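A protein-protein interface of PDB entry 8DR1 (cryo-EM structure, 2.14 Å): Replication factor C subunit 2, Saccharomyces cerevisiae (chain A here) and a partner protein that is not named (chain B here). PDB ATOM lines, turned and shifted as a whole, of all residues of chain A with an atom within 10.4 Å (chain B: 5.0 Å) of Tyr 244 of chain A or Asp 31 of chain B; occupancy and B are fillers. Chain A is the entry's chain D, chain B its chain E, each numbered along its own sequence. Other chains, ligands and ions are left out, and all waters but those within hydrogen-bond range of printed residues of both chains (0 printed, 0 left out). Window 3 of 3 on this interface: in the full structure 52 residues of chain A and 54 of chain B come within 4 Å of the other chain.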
ATOM      1  N   GLN A 236       1.065  34.701  -8.791  1.00  0.00           N
ATOM      2  CA  GLN A 236       1.811  34.965  -7.564  1.00  0.00           C
ATOM      3  C   GLN A 236       1.163  34.277  -6.367  1.00  0.00           C
ATOM      4  O   GLN A 236       1.860  33.720  -5.510  1.00  0.00           O
ATOM      5  CB  GLN A 236       1.919  36.471  -7.318  1.00  0.00           C
ATOM      6  CG  GLN A 236       2.771  36.829  -6.108  1.00  0.00           C
ATOM      7  CD  GLN A 236       2.924  38.325  -5.908  1.00  0.00           C
ATOM      8  OE1 GLN A 236       2.435  39.126  -6.703  1.00  0.00           O
ATOM      9  NE2 GLN A 236       3.609  38.709  -4.837  1.00  0.00           N
ATOM     10  N   SER A 237      -0.169  34.314  -6.282  1.00  0.00           N
ATOM     11  CA  SER A 237      -0.847  33.649  -5.173  1.00  0.00           C
ATOM     12  C   SER A 237      -0.606  32.143  -5.206  1.00  0.00           C
ATOM     13  O   SER A 237      -0.340  31.523  -4.168  1.00  0.00           O
ATOM     14  CB  SER A 237      -2.344  33.962  -5.211  1.00  0.00           C
ATOM     15  OG  SER A 237      -3.079  32.905  -5.800  1.00  0.00           O
ATOM     16  N   ALA A 238      -0.685  31.539  -6.394  1.00  0.00           N
ATOM     17  CA  ALA A 238      -0.423  30.108  -6.512  1.00  0.00           C
ATOM     18  C   ALA A 238       1.018  29.781  -6.139  1.00  0.00           C
ATOM     19  O   ALA A 238       1.286  28.760  -5.492  1.00  0.00           O
ATOM     20  CB  ALA A 238      -0.733  29.633  -7.930  1.00  0.00           C
ATOM     21  N   SER A 239       1.962  30.633  -6.546  1.00  0.00           N
ATOM     22  CA  SER A 239       3.359  30.419  -6.184  1.00  0.00           C
ATOM     23  C   SER A 239       3.553  30.490  -4.676  1.00  0.00           C
ATOM     24  O   SER A 239       4.294  29.688  -4.100  1.00  0.00           O
ATOM     25  CB  SER A 239       4.243  31.452  -6.884  1.00  0.00           C
ATOM     26  OG  SER A 239       5.602  31.286  -6.523  1.00  0.00           O
ATOM     27  N   LYS A 240       2.906  31.456  -4.019  1.00  0.00           N
ATOM     28  CA  LYS A 240       2.995  31.541  -2.566  1.00  0.00           C
ATOM     29  C   LYS A 240       2.437  30.282  -1.914  1.00  0.00           C
ATOM     30  O   LYS A 240       3.026  29.749  -0.965  1.00  0.00           O
ATOM     31  CB  LYS A 240       2.251  32.776  -2.059  1.00  0.00           C
ATOM     32  CG  LYS A 240       2.933  34.096  -2.383  1.00  0.00           C
ATOM     33  CD  LYS A 240       2.411  35.225  -1.506  1.00  0.00           C
ATOM     34  CE  LYS A 240       3.411  36.367  -1.407  1.00  0.00           C
ATOM     35  NZ  LYS A 240       4.636  35.984  -0.648  1.00  0.00           N
ATOM     36  N   GLY A 241       1.298  29.796  -2.408  1.00  0.00           N
ATOM     37  CA  GLY A 241       0.743  28.565  -1.863  1.00  0.00           C
ATOM     38  C   GLY A 241       1.695  27.394  -2.008  1.00  0.00           C
ATOM     39  O   GLY A 241       1.932  26.642  -1.056  1.00  0.00           O
ATOM     40  N   ALA A 242       2.268  27.232  -3.203  1.00  0.00           N
ATOM     41  CA  ALA A 242       3.195  26.127  -3.434  1.00  0.00           C
ATOM     42  C   ALA A 242       4.423  26.242  -2.540  1.00  0.00           C
ATOM     43  O   ALA A 242       4.878  25.244  -1.968  1.00  0.00           O
ATOM     44  CB  ALA A 242       3.606  26.086  -4.905  1.00  0.00           C
ATOM     45  N   GLN A 243       4.974  27.450  -2.408  1.00  0.00           N
ATOM     46  CA  GLN A 243       6.148  27.635  -1.562  1.00  0.00           C
ATOM     47  C   GLN A 243       5.834  27.308  -0.109  1.00  0.00           C
ATOM     48  O   GLN A 243       6.626  26.643   0.569  1.00  0.00           O
ATOM     49  CB  GLN A 243       6.664  29.071  -1.684  1.00  0.00           C
ATOM     50  CG  GLN A 243       7.409  29.390  -2.979  1.00  0.00           C
ATOM     51  CD  GLN A 243       8.364  28.292  -3.410  1.00  0.00           C
ATOM     52  OE1 GLN A 243       7.986  27.379  -4.144  1.00  0.00           O
ATOM     53  NE2 GLN A 243       9.607  28.377  -2.954  1.00  0.00           N
ATOM     54  N   TYR A 244       4.681  27.762   0.389  1.00  0.00           N
ATOM     55  CA  TYR A 244       4.319  27.462   1.769  1.00  0.00           C
ATOM     56  C   TYR A 244       4.149  25.963   1.978  1.00  0.00           C
ATOM     57  O   TYR A 244       4.594  25.417   2.993  1.00  0.00           O
ATOM     58  CB  TYR A 244       3.040  28.198   2.159  1.00  0.00           C
ATOM     59  CG  TYR A 244       2.660  28.000   3.608  1.00  0.00           C
ATOM     60  CD1 TYR A 244       3.395  28.595   4.625  1.00  0.00           C
ATOM     61  CD2 TYR A 244       1.569  27.218   3.961  1.00  0.00           C
ATOM     62  CE1 TYR A 244       3.052  28.418   5.951  1.00  0.00           C
ATOM     63  CE2 TYR A 244       1.220  27.034   5.283  1.00  0.00           C
ATOM     64  CZ  TYR A 244       1.965  27.637   6.274  1.00  0.00           C
ATOM     65  OH  TYR A 244       1.618  27.457   7.594  1.00  0.00           O
ATOM     66  N   LEU A 245       3.501  25.281   1.031  1.00  0.00           N
ATOM     67  CA  LEU A 245       3.340  23.838   1.170  1.00  0.00           C
ATOM     68  C   LEU A 245       4.689  23.134   1.232  1.00  0.00           C
ATOM     69  O   LEU A 245       4.834  22.129   1.937  1.00  0.00           O
ATOM     70  CB  LEU A 245       2.501  23.286   0.016  1.00  0.00           C
ATOM     71  CG  LEU A 245       1.933  21.868   0.166  1.00  0.00           C
ATOM     72  CD1 LEU A 245       1.439  21.592   1.583  1.00  0.00           C
ATOM     73  CD2 LEU A 245       0.814  21.641  -0.838  1.00  0.00           C
ATOM     74  N   GLY A 246       5.683  23.640   0.504  1.00  0.00           N
ATOM     75  CA  GLY A 246       7.027  23.102   0.572  1.00  0.00           C
ATOM     76  C   GLY A 246       7.103  21.629   0.229  1.00  0.00           C
ATOM     77  O   GLY A 246       7.771  20.858   0.923  1.00  0.00           O
ATOM     78  N   ASP A 247       6.423  21.228  -0.844  1.00  0.00           N
ATOM     79  CA  ASP A 247       6.384  19.835  -1.270  1.00  0.00           C
ATOM     80  C   ASP A 247       7.131  19.576  -2.568  1.00  0.00           C
ATOM     81  O   ASP A 247       7.608  18.458  -2.777  1.00  0.00           O
ATOM     82  CB  ASP A 247       4.929  19.377  -1.440  1.00  0.00           C
ATOM     83  CG  ASP A 247       4.791  17.867  -1.476  1.00  0.00           C
ATOM     84  OD1 ASP A 247       5.826  17.169  -1.509  1.00  0.00           O
ATOM     85  OD2 ASP A 247       3.642  17.378  -1.473  1.00  0.00           O
ATOM     86  N   GLY A 248       7.251  20.576  -3.439  1.00  0.00           N
ATOM     87  CA  GLY A 248       7.875  20.401  -4.731  1.00  0.00           C
ATOM     88  C   GLY A 248       6.937  19.949  -5.827  1.00  0.00           C
ATOM     89  O   GLY A 248       7.353  19.888  -6.991  1.00  0.00           O
ATOM     90  N   LYS A 249       5.689  19.628  -5.497  1.00  0.00           N
ATOM     91  CA  LYS A 249       4.726  19.220  -6.506  1.00  0.00           C
ATOM     92  C   LYS A 249       4.351  20.402  -7.394  1.00  0.00           C
ATOM     93  O   LYS A 249       4.316  21.554  -6.956  1.00  0.00           O
ATOM     94  CB  LYS A 249       3.470  18.647  -5.847  1.00  0.00           C
ATOM     95  CG  LYS A 249       3.740  17.514  -4.864  1.00  0.00           C
ATOM     96  CD  LYS A 249       3.971  16.195  -5.581  1.00  0.00           C
ATOM     97  CE  LYS A 249       2.660  15.530  -5.969  1.00  0.00           C
ATOM     98  NZ  LYS A 249       1.909  15.030  -4.785  1.00  0.00           N
ATOM     99  N   ILE A 251       2.147  22.994  -9.600  1.00  0.00           N
ATOM    100  CA  ILE A 251       0.849  23.631  -9.424  1.00  0.00           C
ATOM    101  C   ILE A 251      -0.146  23.019 -10.401  1.00  0.00           C
ATOM    102  O   ILE A 251       0.174  22.773 -11.571  1.00  0.00           O
ATOM    103  CB  ILE A 251       0.959  25.152  -9.623  1.00  0.00           C
ATOM    104  CG1 ILE A 251       1.733  25.788  -8.467  1.00  0.00           C
ATOM    105  CG2 ILE A 251      -0.424  25.779  -9.726  1.00  0.00           C
ATOM    106  CD1 ILE A 251       2.640  26.918  -8.894  1.00  0.00           C
ATOM    107  N   GLN A 255      -5.956  23.912  -8.117  1.00  0.00           N
ATOM    108  CA  GLN A 255      -5.512  24.950  -7.194  1.00  0.00           C
ATOM    109  C   GLN A 255      -5.769  26.336  -7.770  1.00  0.00           C
ATOM    110  O   GLN A 255      -6.219  27.241  -7.057  1.00  0.00           O
ATOM    111  CB  GLN A 255      -4.028  24.769  -6.877  1.00  0.00           C
ATOM    112  CG  GLN A 255      -3.753  23.827  -5.719  1.00  0.00           C
ATOM    113  CD  GLN A 255      -2.503  22.995  -5.930  1.00  0.00           C
ATOM    114  OE1 GLN A 255      -2.550  21.766  -5.902  1.00  0.00           O
ATOM    115  NE2 GLN A 255      -1.377  23.665  -6.146  1.00  0.00           N
ATOM    116  N   ASN B  24      -5.091  28.010   6.258  1.00  0.00           N
ATOM    117  CA  ASN B  24      -3.830  27.621   5.636  1.00  0.00           C
ATOM    118  C   ASN B  24      -3.439  28.598   4.533  1.00  0.00           C
ATOM    119  O   ASN B  24      -2.261  28.942   4.388  1.00  0.00           O
ATOM    120  CB  ASN B  24      -3.931  26.200   5.083  1.00  0.00           C
ATOM    121  CG  ASN B  24      -4.138  25.163   6.170  1.00  0.00           C
ATOM    122  OD1 ASN B  24      -3.677  25.330   7.299  1.00  0.00           O
ATOM    123  ND2 ASN B  24      -4.831  24.083   5.834  1.00  0.00           N
ATOM    124  N   LYS B  27      -2.079  31.681   6.165  1.00  0.00           N
ATOM    125  CA  LYS B  27      -0.732  31.412   6.657  1.00  0.00           C
ATOM    126  C   LYS B  27       0.279  31.431   5.519  1.00  0.00           C
ATOM    127  O   LYS B  27       1.386  31.963   5.669  1.00  0.00           O
ATOM    128  CB  LYS B  27      -0.693  30.067   7.385  1.00  0.00           C
ATOM    129  CG  LYS B  27      -1.322  30.099   8.766  1.00  0.00           C
ATOM    130  CD  LYS B  27      -1.446  28.706   9.359  1.00  0.00           C
ATOM    131  CE  LYS B  27      -1.999  28.755  10.773  1.00  0.00           C
ATOM    132  NZ  LYS B  27      -2.199  27.396  11.345  1.00  0.00           N
ATOM    133  N   SER B  28      -0.084  30.858   4.370  1.00  0.00           N
ATOM    134  CA  SER B  28       0.800  30.905   3.209  1.00  0.00           C
ATOM    135  C   SER B  28       1.043  32.342   2.766  1.00  0.00           C
ATOM    136  O   SER B  28       2.162  32.701   2.381  1.00  0.00           O
ATOM    137  CB  SER B  28       0.204  30.085   2.064  1.00  0.00           C
ATOM    138  OG  SER B  28      -0.676  30.867   1.278  1.00  0.00           O
ATOM    139  N   LEU B  29       0.003  33.177   2.806  1.00  0.00           N
ATOM    140  CA  LEU B  29       0.184  34.586   2.470  1.00  0.00           C
ATOM    141  C   LEU B  29       1.141  35.265   3.442  1.00  0.00           C
ATOM    142  O   LEU B  29       1.972  36.086   3.038  1.00  0.00           O
ATOM    143  CB  LEU B  29      -1.164  35.311   2.465  1.00  0.00           C
ATOM    144  CG  LEU B  29      -2.079  35.111   1.254  1.00  0.00           C
ATOM    145  CD1 LEU B  29      -3.331  35.959   1.413  1.00  0.00           C
ATOM    146  CD2 LEU B  29      -1.367  35.445  -0.049  1.00  0.00           C
ATOM    147  N   SER B  30       1.040  34.935   4.730  1.00  0.00           N
ATOM    148  CA  SER B  30       1.869  35.572   5.746  1.00  0.00           C
ATOM    149  C   SER B  30       3.275  34.988   5.828  1.00  0.00           C
ATOM    150  O   SER B  30       4.100  35.518   6.580  1.00  0.00           O
ATOM    151  CB  SER B  30       1.196  35.458   7.115  1.00  0.00           C
ATOM    152  OG  SER B  30       1.329  34.149   7.641  1.00  0.00           O
ATOM    153  N   ASP B  31       3.568  33.920   5.086  1.00  0.00           N
ATOM    154  CA  ASP B  31       4.889  33.304   5.171  1.00  0.00           C
ATOM    155  C   ASP B  31       5.980  34.253   4.683  1.00  0.00           C
ATOM    156  O   ASP B  31       7.042  34.358   5.307  1.00  0.00           O
ATOM    157  CB  ASP B  31       4.911  32.004   4.370  1.00  0.00           C
ATOM    158  CG  ASP B  31       6.273  31.344   4.367  1.00  0.00           C
ATOM    159  OD1 ASP B  31       6.765  30.991   5.459  1.00  0.00           O
ATOM    160  OD2 ASP B  31       6.853  31.176   3.274  1.00  0.00           O
ATOM    161  N   GLN B  32       5.738  34.947   3.572  1.00  0.00           N
ATOM    162  CA  GLN B  32       6.688  35.902   2.996  1.00  0.00           C
ATOM    163  C   GLN B  32       5.940  37.204   2.747  1.00  0.00           C
ATOM    164  O   GLN B  32       5.525  37.493   1.617  1.00  0.00           O
ATOM    165  CB  GLN B  32       7.318  35.364   1.709  1.00  0.00           C
ATOM    166  CG  GLN B  32       7.590  33.863   1.697  1.00  0.00           C
ATOM    167  CD  GLN B  32       8.941  33.512   2.287  1.00  0.00           C
ATOM    168  OE1 GLN B  32       9.282  33.945   3.388  1.00  0.00           O
ATOM    169  NE2 GLN B  32       9.719  32.721   1.556  1.00  0.00           N
ATOM    170  N   PRO B  33       5.752  38.024   3.786  1.00  0.00           N
ATOM    171  CA  PRO B  33       4.865  39.189   3.661  1.00  0.00           C
ATOM    172  C   PRO B  33       5.464  40.384   2.933  1.00  0.00           C
ATOM    173  O   PRO B  33       4.735  41.356   2.689  1.00  0.00           O
ATOM    174  CB  PRO B  33       4.563  39.544   5.122  1.00  0.00           C
ATOM    175  CG  PRO B  33       5.780  39.110   5.860  1.00  0.00           C
ATOM    176  CD  PRO B  33       6.278  37.876   5.156  1.00  0.00           C
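Tyr 244 of chain A touches just these residues of chain B: Lys 27 (3.5 Å), Ser 28 (3.4 Å) and Asp 31 (3.7 Å).
Asp 31 of chain B touches just one residue of chain A: Tyr 244 (3.7 Å).
Of chain A, only Tyr 244 comes within 4 Å of Lys 27 of chain B.
No residue of chain A comes within 4 Å of Ser 30 of chain B.
Gln 32 of chain B touches just one residue of chain A: Lys 240 (2.9 Å).
Printed residues of chain B within 4 Å of Lys 240 of chain A: Gln 32 (2.9 Å).
The nearest residue of chain A that does not touch Asp 31 of chain B is Gln 243 of chain A (5.2 Å).
The nearest printed residue of chain B that does not touch Lys 240 of chain A is Leu 29 of chain B (4.1 Å).
The backbone carbonyl oxygen (O) of Lys 27 of chain B is in hydrogen-bond range of the side-chain hydroxyl (OG) of Ser 30 of chain B (2.9 Å).
Of the 16 printed residues of chain A, 2 touch a printed residue of chain B.
Among the printed residues, no Asp or Glu carboxylate lies within 4 Å of a Lys or Arg side-chain nitrogen of the other chain.
NZ of Lys 240 of chain A sits at hydrogen-bond distance from O of Gln 32 of chain B (2.9 Å).
Tyr 244 of chain A touches Lys 27 of chain B (OH to CB, 3.5 Å).
CB of Ser 28 of chain B touches CB of Tyr 244 of chain A, 3.4 Å away.
Asp 31 of chain B touches Tyr 244 of chain A.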
